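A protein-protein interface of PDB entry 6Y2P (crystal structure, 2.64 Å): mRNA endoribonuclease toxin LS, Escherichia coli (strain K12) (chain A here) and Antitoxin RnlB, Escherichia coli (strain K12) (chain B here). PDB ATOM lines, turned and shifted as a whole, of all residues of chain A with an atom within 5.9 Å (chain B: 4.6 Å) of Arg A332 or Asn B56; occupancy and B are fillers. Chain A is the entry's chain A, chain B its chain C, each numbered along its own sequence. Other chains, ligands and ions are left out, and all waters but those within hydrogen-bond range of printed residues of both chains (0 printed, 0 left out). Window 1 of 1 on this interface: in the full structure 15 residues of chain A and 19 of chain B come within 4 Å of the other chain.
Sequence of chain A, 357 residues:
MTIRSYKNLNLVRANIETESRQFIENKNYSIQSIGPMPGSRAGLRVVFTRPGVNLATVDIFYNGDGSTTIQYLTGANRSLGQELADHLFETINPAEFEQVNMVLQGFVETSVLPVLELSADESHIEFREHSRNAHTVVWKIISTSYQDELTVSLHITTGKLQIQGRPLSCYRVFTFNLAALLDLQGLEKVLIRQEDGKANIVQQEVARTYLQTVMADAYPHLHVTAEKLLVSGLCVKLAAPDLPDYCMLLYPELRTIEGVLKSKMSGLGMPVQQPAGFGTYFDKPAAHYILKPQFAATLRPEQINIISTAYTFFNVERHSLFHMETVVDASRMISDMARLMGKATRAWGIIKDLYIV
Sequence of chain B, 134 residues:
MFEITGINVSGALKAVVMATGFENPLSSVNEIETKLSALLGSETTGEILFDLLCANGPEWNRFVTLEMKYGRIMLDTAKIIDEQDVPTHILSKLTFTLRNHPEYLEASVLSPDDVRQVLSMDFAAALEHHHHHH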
ATOM      1  N   ASP A 245       7.109 -29.375  12.015  1.00  0.00           N
ATOM      2  CA  ASP A 245       6.255 -28.813  13.060  1.00  0.00           C
ATOM      3  C   ASP A 245       7.070 -28.642  14.343  1.00  0.00           C
ATOM      4  O   ASP A 245       7.996 -29.414  14.617  1.00  0.00           O
ATOM      5  CB  ASP A 245       5.022 -29.680  13.345  1.00  0.00           C
ATOM      6  CG  ASP A 245       4.092 -29.030  14.360  1.00  0.00           C
ATOM      7  OD1 ASP A 245       3.336 -28.111  13.949  1.00  0.00           O
ATOM      8  OD2 ASP A 245       4.126 -29.422  15.553  1.00  0.00           O
ATOM      9  N   CYS A 247       5.385 -27.751  17.658  1.00  0.00           N
ATOM     10  CA  CYS A 247       4.631 -27.873  18.914  1.00  0.00           C
ATOM     11  C   CYS A 247       5.399 -28.663  19.984  1.00  0.00           C
ATOM     12  O   CYS A 247       5.405 -28.311  21.182  1.00  0.00           O
ATOM     13  CB  CYS A 247       3.300 -28.560  18.595  1.00  0.00           C
ATOM     14  SG  CYS A 247       2.277 -27.653  17.371  1.00  0.00           S
ATOM     15  N   LEU A 250       7.324 -26.663  22.359  1.00  0.00           N
ATOM     16  CA  LEU A 250       6.641 -25.933  23.410  1.00  0.00           C
ATOM     17  C   LEU A 250       6.130 -26.838  24.526  1.00  0.00           C
ATOM     18  O   LEU A 250       5.767 -26.324  25.587  1.00  0.00           O
ATOM     19  CB  LEU A 250       5.488 -25.125  22.825  1.00  0.00           C
ATOM     20  CG  LEU A 250       5.136 -23.940  23.700  1.00  0.00           C
ATOM     21  CD1 LEU A 250       6.226 -22.855  23.703  1.00  0.00           C
ATOM     22  CD2 LEU A 250       3.792 -23.361  23.257  1.00  0.00           C
ATOM     23  N   VAL A 316      -5.101 -21.267  27.447  1.00  0.00           N
ATOM     24  CA  VAL A 316      -5.246 -20.820  26.071  1.00  0.00           C
ATOM     25  C   VAL A 316      -4.346 -21.637  25.146  1.00  0.00           C
ATOM     26  O   VAL A 316      -4.823 -22.174  24.154  1.00  0.00           O
ATOM     27  CB  VAL A 316      -4.979 -19.298  25.976  1.00  0.00           C
ATOM     28  CG1 VAL A 316      -4.810 -18.817  24.516  1.00  0.00           C
ATOM     29  CG2 VAL A 316      -6.133 -18.553  26.602  1.00  0.00           C
ATOM     30  N   GLU A 317      -3.062 -21.831  25.502  1.00  0.00           N
ATOM     31  CA  GLU A 317      -2.122 -22.535  24.620  1.00  0.00           C
ATOM     32  C   GLU A 317      -2.301 -24.063  24.630  1.00  0.00           C
ATOM     33  O   GLU A 317      -2.251 -24.713  23.570  1.00  0.00           O
ATOM     34  CB  GLU A 317      -0.685 -22.183  25.011  1.00  0.00           C
ATOM     35  CG  GLU A 317      -0.329 -20.719  24.901  1.00  0.00           C
ATOM     36  CD  GLU A 317      -0.400 -20.201  23.462  1.00  0.00           C
ATOM     37  OE1 GLU A 317      -0.395 -18.964  23.234  1.00  0.00           O
ATOM     38  OE2 GLU A 317      -0.483 -21.051  22.558  1.00  0.00           O
ATOM     39  N   ARG A 318      -2.470 -24.658  25.809  1.00  0.00           N
ATOM     40  CA  ARG A 318      -2.663 -26.091  25.972  1.00  0.00           C
ATOM     41  C   ARG A 318      -3.892 -26.585  25.232  1.00  0.00           C
ATOM     42  O   ARG A 318      -3.898 -27.719  24.762  1.00  0.00           O
ATOM     43  CB  ARG A 318      -2.832 -26.381  27.467  1.00  0.00           C
ATOM     44  CG  ARG A 318      -2.125 -27.604  27.983  1.00  0.00           C
ATOM     45  CD  ARG A 318      -2.757 -28.070  29.328  1.00  0.00           C
ATOM     46  NE  ARG A 318      -4.026 -28.792  29.136  1.00  0.00           N
ATOM     47  CZ  ARG A 318      -4.178 -30.120  29.211  1.00  0.00           C
ATOM     48  NH1 ARG A 318      -3.144 -30.901  29.507  1.00  0.00           N
ATOM     49  NH2 ARG A 318      -5.378 -30.672  29.006  1.00  0.00           N
ATOM     50  N   SER A 320      -5.351 -26.370  22.360  1.00  0.00           N
ATOM     51  CA  SER A 320      -5.096 -27.122  21.159  1.00  0.00           C
ATOM     52  C   SER A 320      -3.694 -27.722  21.085  1.00  0.00           C
ATOM     53  O   SER A 320      -3.557 -28.801  20.496  1.00  0.00           O
ATOM     54  CB  SER A 320      -5.391 -26.253  19.922  1.00  0.00           C
ATOM     55  OG  SER A 320      -6.783 -25.935  19.881  1.00  0.00           O
ATOM     56  N   LEU A 321      -2.666 -27.138  21.723  1.00  0.00           N
ATOM     57  CA  LEU A 321      -1.367 -27.805  21.546  1.00  0.00           C
ATOM     58  C   LEU A 321      -1.295 -29.179  22.227  1.00  0.00           C
ATOM     59  O   LEU A 321      -0.557 -30.049  21.750  1.00  0.00           O
ATOM     60  CB  LEU A 321      -0.217 -26.923  22.026  1.00  0.00           C
ATOM     61  CG  LEU A 321      -0.205 -25.630  21.206  1.00  0.00           C
ATOM     62  CD1 LEU A 321       0.908 -24.727  21.639  1.00  0.00           C
ATOM     63  CD2 LEU A 321       0.001 -25.958  19.732  1.00  0.00           C
ATOM     64  N   HIS A 323      -3.889 -31.338  22.443  1.00  0.00           N
ATOM     65  CA  HIS A 323      -5.083 -32.064  22.027  1.00  0.00           C
ATOM     66  C   HIS A 323      -5.102 -32.116  20.502  1.00  0.00           C
ATOM     67  O   HIS A 323      -4.172 -31.637  19.831  1.00  0.00           O
ATOM     68  CB  HIS A 323      -6.368 -31.400  22.569  1.00  0.00           C
ATOM     69  CG  HIS A 323      -6.534 -31.527  24.050  1.00  0.00           C
ATOM     70  ND1 HIS A 323      -7.032 -32.663  24.644  1.00  0.00           N
ATOM     71  CD2 HIS A 323      -6.240 -30.677  25.066  1.00  0.00           C
ATOM     72  CE1 HIS A 323      -7.060 -32.504  25.956  1.00  0.00           C
ATOM     73  NE2 HIS A 323      -6.565 -31.316  26.239  1.00  0.00           N
ATOM     74  N   GLU A 325      -8.257 -32.140  17.096  1.00  0.00           N
ATOM     75  CA  GLU A 325      -9.649 -32.133  16.709  1.00  0.00           C
ATOM     76  C   GLU A 325     -10.044 -33.469  16.082  1.00  0.00           C
ATOM     77  O   GLU A 325      -9.219 -34.186  15.513  1.00  0.00           O
ATOM     78  CB  GLU A 325      -9.870 -31.020  15.698  1.00  0.00           C
ATOM     79  CG  GLU A 325      -9.507 -29.695  16.215  1.00  0.00           C
ATOM     80  CD  GLU A 325     -10.529 -29.251  17.211  1.00  0.00           C
ATOM     81  OE1 GLU A 325     -11.710 -29.592  16.975  1.00  0.00           O
ATOM     82  OE2 GLU A 325     -10.156 -28.590  18.218  1.00  0.00           O
ATOM     83  N   ASP A 329      -7.122 -32.709  10.590  1.00  0.00           N
ATOM     84  CA  ASP A 329      -6.304 -31.731   9.884  1.00  0.00           C
ATOM     85  C   ASP A 329      -6.587 -30.293  10.301  1.00  0.00           C
ATOM     86  O   ASP A 329      -5.857 -29.387   9.891  1.00  0.00           O
ATOM     87  CB  ASP A 329      -6.514 -31.882   8.381  1.00  0.00           C
ATOM     88  CG  ASP A 329      -5.810 -33.106   7.820  1.00  0.00           C
ATOM     89  OD1 ASP A 329      -4.812 -33.531   8.457  1.00  0.00           O
ATOM     90  OD2 ASP A 329      -6.267 -33.623   6.756  1.00  0.00           O
ATOM     91  N   ALA A 330      -7.614 -30.036  11.090  1.00  0.00           N
ATOM     92  CA  ALA A 330      -7.829 -28.687  11.598  1.00  0.00           C
ATOM     93  C   ALA A 330      -7.159 -28.435  12.951  1.00  0.00           C
ATOM     94  O   ALA A 330      -7.279 -27.327  13.484  1.00  0.00           O
ATOM     95  CB  ALA A 330      -9.329 -28.396  11.680  1.00  0.00           C
ATOM     96  N   SER A 331      -6.415 -29.402  13.483  1.00  0.00           N
ATOM     97  CA  SER A 331      -5.682 -29.235  14.737  1.00  0.00           C
ATOM     98  C   SER A 331      -4.539 -28.218  14.634  1.00  0.00           C
ATOM     99  O   SER A 331      -3.936 -28.010  13.572  1.00  0.00           O
ATOM    100  CB  SER A 331      -5.149 -30.591  15.214  1.00  0.00           C
ATOM    101  OG  SER A 331      -6.192 -31.560  15.168  1.00  0.00           O
ATOM    102  N   ARG A 332      -4.255 -27.575  15.767  1.00  0.00           N
ATOM    103  CA  ARG A 332      -3.329 -26.460  15.787  1.00  0.00           C
ATOM    104  C   ARG A 332      -1.917 -26.982  15.611  1.00  0.00           C
ATOM    105  O   ARG A 332      -1.509 -27.925  16.297  1.00  0.00           O
ATOM    106  CB  ARG A 332      -3.466 -25.656  17.091  1.00  0.00           C
ATOM    107  CG  ARG A 332      -2.308 -24.673  17.376  1.00  0.00           C
ATOM    108  CD  ARG A 332      -2.718 -23.585  18.284  1.00  0.00           C
ATOM    109  NE  ARG A 332      -1.671 -22.589  18.499  1.00  0.00           N
ATOM    110  CZ  ARG A 332      -1.303 -22.120  19.691  1.00  0.00           C
ATOM    111  NH1 ARG A 332      -1.872 -22.579  20.804  1.00  0.00           N
ATOM    112  NH2 ARG A 332      -0.367 -21.180  19.773  1.00  0.00           N
ATOM    113  N   MET A 333      -1.174 -26.359  14.688  1.00  0.00           N
ATOM    114  CA  MET A 333       0.229 -26.632  14.414  1.00  0.00           C
ATOM    115  C   MET A 333       1.011 -25.325  14.542  1.00  0.00           C
ATOM    116  O   MET A 333       0.444 -24.221  14.464  1.00  0.00           O
ATOM    117  CB  MET A 333       0.422 -27.197  12.998  1.00  0.00           C
ATOM    118  CG  MET A 333      -0.513 -28.310  12.635  1.00  0.00           C
ATOM    119  SD  MET A 333      -0.038 -29.842  13.521  1.00  0.00           S
ATOM    120  CE  MET A 333       1.414 -30.350  12.600  1.00  0.00           C
ATOM    121  N   ILE A 334       2.330 -25.458  14.686  1.00  0.00           N
ATOM    122  CA  ILE A 334       3.263 -24.347  14.591  1.00  0.00           C
ATOM    123  C   ILE A 334       4.382 -24.700  13.604  1.00  0.00           C
ATOM    124  O   ILE A 334       5.282 -25.478  13.938  1.00  0.00           O
ATOM    125  CB  ILE A 334       3.858 -23.998  15.941  1.00  0.00           C
ATOM    126  CG1 ILE A 334       2.743 -23.779  16.952  1.00  0.00           C
ATOM    127  CG2 ILE A 334       4.689 -22.730  15.797  1.00  0.00           C
ATOM    128  CD1 ILE A 334       3.299 -23.312  18.322  1.00  0.00           C
ATOM    129  N   LYS A 343       6.382 -17.748  21.785  1.00  0.00           N
ATOM    130  CA  LYS A 343       5.543 -18.368  22.790  1.00  0.00           C
ATOM    131  C   LYS A 343       6.379 -18.853  23.954  1.00  0.00           C
ATOM    132  O   LYS A 343       6.008 -18.667  25.123  1.00  0.00           O
ATOM    133  CB  LYS A 343       4.752 -19.499  22.163  1.00  0.00           C
ATOM    134  CG  LYS A 343       3.832 -19.047  21.051  1.00  0.00           C
ATOM    135  CD  LYS A 343       2.650 -18.363  21.633  1.00  0.00           C
ATOM    136  CE  LYS A 343       1.648 -17.974  20.579  1.00  0.00           C
ATOM    137  NZ  LYS A 343       0.346 -17.596  21.153  1.00  0.00           N
ATOM    138  N   ASN B  24     -11.668 -24.118  18.848  1.00  0.00           N
ATOM    139  CA  ASN B  24     -11.871 -24.493  17.456  1.00  0.00           C
ATOM    140  C   ASN B  24     -13.362 -24.682  17.166  1.00  0.00           C
ATOM    141  O   ASN B  24     -13.990 -25.575  17.757  1.00  0.00           O
ATOM    142  CB  ASN B  24     -11.117 -25.770  17.145  1.00  0.00           C
ATOM    143  CG  ASN B  24     -10.834 -25.916  15.672  1.00  0.00           C
ATOM    144  OD1 ASN B  24     -11.724 -25.670  14.841  1.00  0.00           O
ATOM    145  ND2 ASN B  24      -9.575 -26.324  15.317  1.00  0.00           N
ATOM    146  N   LEU B  52      -9.931 -20.563  10.641  1.00  0.00           N
ATOM    147  CA  LEU B  52      -9.646 -20.904  12.027  1.00  0.00           C
ATOM    148  C   LEU B  52      -8.555 -20.039  12.657  1.00  0.00           C
ATOM    149  O   LEU B  52      -7.975 -20.439  13.693  1.00  0.00           O
ATOM    150  CB  LEU B  52      -9.280 -22.381  12.125  1.00  0.00           C
ATOM    151  CG  LEU B  52     -10.192 -23.377  11.386  1.00  0.00           C
ATOM    152  CD1 LEU B  52      -9.615 -24.807  11.416  1.00  0.00           C
ATOM    153  CD2 LEU B  52     -11.579 -23.395  12.006  1.00  0.00           C
ATOM    154  N   LEU B  53      -8.333 -18.830  12.114  1.00  0.00           N
ATOM    155  CA  LEU B  53      -7.183 -18.007  12.506  1.00  0.00           C
ATOM    156  C   LEU B  53      -7.072 -17.851  14.024  1.00  0.00           C
ATOM    157  O   LEU B  53      -5.993 -18.043  14.599  1.00  0.00           O
ATOM    158  CB  LEU B  53      -7.265 -16.631  11.855  1.00  0.00           C
ATOM    159  CG  LEU B  53      -6.210 -15.663  12.408  1.00  0.00           C
ATOM    160  CD1 LEU B  53      -4.873 -16.127  11.912  1.00  0.00           C
ATOM    161  CD2 LEU B  53      -6.443 -14.183  12.082  1.00  0.00           C
ATOM    162  N   CYS B  54      -8.185 -17.548  14.701  1.00  0.00           N
ATOM    163  CA  CYS B  54      -8.063 -17.284  16.129  1.00  0.00           C
ATOM    164  C   CYS B  54      -7.865 -18.553  16.953  1.00  0.00           C
ATOM    165  O   CYS B  54      -7.340 -18.477  18.071  1.00  0.00           O
ATOM    166  CB  CYS B  54      -9.330 -16.590  16.646  1.00  0.00           C
ATOM    167  SG  CYS B  54      -9.595 -14.879  16.022  1.00  0.00           S
ATOM    168  N   ALA B  55      -8.056 -19.726  16.369  1.00  0.00           N
ATOM    169  CA  ALA B  55      -7.712 -20.914  17.118  1.00  0.00           C
ATOM    170  C   ALA B  55      -6.384 -21.499  16.677  1.00  0.00           C
ATOM    171  O   ALA B  55      -5.661 -22.097  17.486  1.00  0.00           O
ATOM    172  CB  ALA B  55      -8.810 -21.965  16.954  1.00  0.00           C
ATOM    173  N   ASN B  56      -6.034 -21.268  15.412  1.00  0.00           N
ATOM    174  CA  ASN B  56      -4.907 -21.921  14.797  1.00  0.00           C
ATOM    175  C   ASN B  56      -3.734 -21.003  14.497  1.00  0.00           C
ATOM    176  O   ASN B  56      -2.637 -21.501  14.254  1.00  0.00           O
ATOM    177  CB  ASN B  56      -5.403 -22.601  13.520  1.00  0.00           C
ATOM    178  CG  ASN B  56      -5.943 -24.017  13.799  1.00  0.00           C
ATOM    179  OD1 ASN B  56      -5.899 -24.504  14.951  1.00  0.00           O
ATOM    180  ND2 ASN B  56      -6.415 -24.691  12.756  1.00  0.00           N
ATOM    181  N   GLY B  57      -3.882 -19.698  14.644  1.00  0.00           N
ATOM    182  CA  GLY B  57      -2.847 -18.793  14.200  1.00  0.00           C
ATOM    183  C   GLY B  57      -2.790 -18.697  12.681  1.00  0.00           C
ATOM    184  O   GLY B  57      -3.530 -19.382  11.961  1.00  0.00           O
ATOM    185  N   PRO B  58      -1.880 -17.868  12.158  1.00  0.00           N
ATOM    186  CA  PRO B  58      -1.748 -17.713  10.698  1.00  0.00           C
ATOM    187  C   PRO B  58      -0.932 -18.847  10.073  1.00  0.00           C
ATOM    188  O   PRO B  58       0.159 -18.635   9.533  1.00  0.00           O
ATOM    189  CB  PRO B  58      -1.048 -16.358  10.588  1.00  0.00           C
ATOM    190  CG  PRO B  58      -0.095 -16.407  11.735  1.00  0.00           C
ATOM    191  CD  PRO B  58      -0.742 -17.244  12.851  1.00  0.00           C
ATOM    192  N   GLU B  59      -1.454 -20.075  10.168  1.00  0.00           N
ATOM    193  CA  GLU B  59      -0.723 -21.291   9.854  1.00  0.00           C
ATOM    194  C   GLU B  59      -1.213 -21.887   8.535  1.00  0.00           C
ATOM    195  O   GLU B  59      -2.182 -21.409   7.938  1.00  0.00           O
ATOM    196  CB  GLU B  59      -0.853 -22.303  10.992  1.00  0.00           C
ATOM    197  CG  GLU B  59       0.185 -22.111  12.092  1.00  0.00           C
ATOM    198  CD  GLU B  59       1.598 -22.323  11.557  1.00  0.00           C
ATOM    199  OE1 GLU B  59       1.731 -22.966  10.490  1.00  0.00           O
ATOM    200  OE2 GLU B  59       2.569 -21.838  12.174  1.00  0.00           O
ATOM    201  N   ASN B  61      -2.743 -24.598   7.926  1.00  0.00           N
ATOM    202  CA  ASN B  61      -4.093 -25.158   8.023  1.00  0.00           C
ATOM    203  C   ASN B  61      -5.050 -24.168   8.689  1.00  0.00           C
ATOM    204  O   ASN B  61      -5.900 -24.537   9.505  1.00  0.00           O
ATOM    205  CB  ASN B  61      -4.091 -26.494   8.766  1.00  0.00           C
ATOM    206  CG  ASN B  61      -3.706 -26.350  10.219  1.00  0.00           C
ATOM    207  OD1 ASN B  61      -3.208 -25.293  10.646  1.00  0.00           O
ATOM    208  ND2 ASN B  61      -3.912 -27.423  10.995  1.00  0.00           N
ATOM    209  N   VAL B 109      -5.234 -17.151  19.834  1.00  0.00           N
ATOM    210  CA  VAL B 109      -3.883 -17.612  20.081  1.00  0.00           C
ATOM    211  C   VAL B 109      -2.843 -16.718  19.409  1.00  0.00           C
ATOM    212  O   VAL B 109      -1.642 -16.965  19.581  1.00  0.00           O
ATOM    213  CB  VAL B 109      -3.746 -19.094  19.665  1.00  0.00           C
ATOM    214  CG1 VAL B 109      -4.665 -19.945  20.503  1.00  0.00           C
ATOM    215  CG2 VAL B 109      -4.039 -19.283  18.188  1.00  0.00           C
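The side-chain amino group (NZ) of Lys A343 lies within hydrogen-bond range of the backbone carbonyl oxygen (O) of Val B109 (2.6 Å).
The backbone carbonyl oxygen of Ala A330 sits at hydrogen-bond distance from the side-chain amide nitrogen of Asn B24 (3.1 Å).
O of Asp A329 sits at hydrogen-bond distance from ND2 of Asn B61, at 3.0 Å.
The backbone carbonyl oxygen of Ala A330 is in hydrogen-bond range of the side-chain amide nitrogen of Asn B56, at 2.9 Å.
The backbone carbonyl oxygen of Ser A331 sits at hydrogen-bond distance from the side-chain amide nitrogen of Asn B61, at 2.6 Å.
The side-chain amino group (NZ) of Lys A343 is in salt-bridge range of the side-chain carboxylate (OE1) of Glu A317 (2.6 Å).
OD1 of Asp A245 is in hydrogen-bond range of N of Ile A334.
The side-chain amide nitrogen (ND2) of Asn B56 lies within hydrogen-bond range of the backbone carbonyl oxygen (O) of Asn B61 (3.3 Å).
The backbone carbonyl oxygen (O) of Cys B54 sits at hydrogen-bond distance from the backbone NH (N) of Val B109, at 3.0 Å.
The backbone NH of Glu A325 is in hydrogen-bond range of the side-chain hydroxyl of Ser A331.
OE2 of Glu A317 is in salt-bridge range of NH1 of Arg A332, 2.7 Å away.
Among the printed residues, pairs that only touch across the chains: Glu A325 with Asn B24 (3.2 Å), Ala A330 with Leu B52 (3.6 Å), Ala A330 with Asn B61 (3.9 Å), Ser A331 with Asn B56 (3.97 Å), Arg A332 with Ala B55 (3.4 Å), Arg A332 with Asn B56 (3.3 Å), Arg A332 with Val B109 (3.9 Å), Met A333 with Glu B59 (3.2 Å), Met A333 with Asn B61 (3.9 Å) and Ile A334 with Glu B59 (3.6 Å).
Arg A332 touches just these residues of chain B: Ala B55, Asn B56 and Val B109.
Of chain A, only Ala A330 (2.9 Å), Ser A331 (3.97 Å) and Arg A332 (3.3 Å) come within 4 Å of Asn B56.
Of the printed residues of chain B, Ala A330 touches Asn B24 (3.1 Å), Leu B52 (3.6 Å), Asn B56 (2.9 Å) and Asn B61 (3.9 Å).
Of the printed residues of chain B, Lys A343 touches Val B109 (2.6 Å).
The nearest printed residue of chain B that does not touch Arg A332 is Asn B61 (4.8 Å).
The nearest residue of chain A that does not touch Asn B56 is Met A333 (4.1 Å).
The nearest printed residue of chain B that does not touch Ile A334 is Asn B56 (6.4 Å).
Along chain A the printed residues that touch a printed residue of chain B span positions 325 to 343.
Of the 11 printed residues of chain B, 7 touch a printed residue of chain A.
Hydrophobic or aromatic side chains of chain B within 4 Å of the printed part of chain A: Leu B52 and Val B109.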
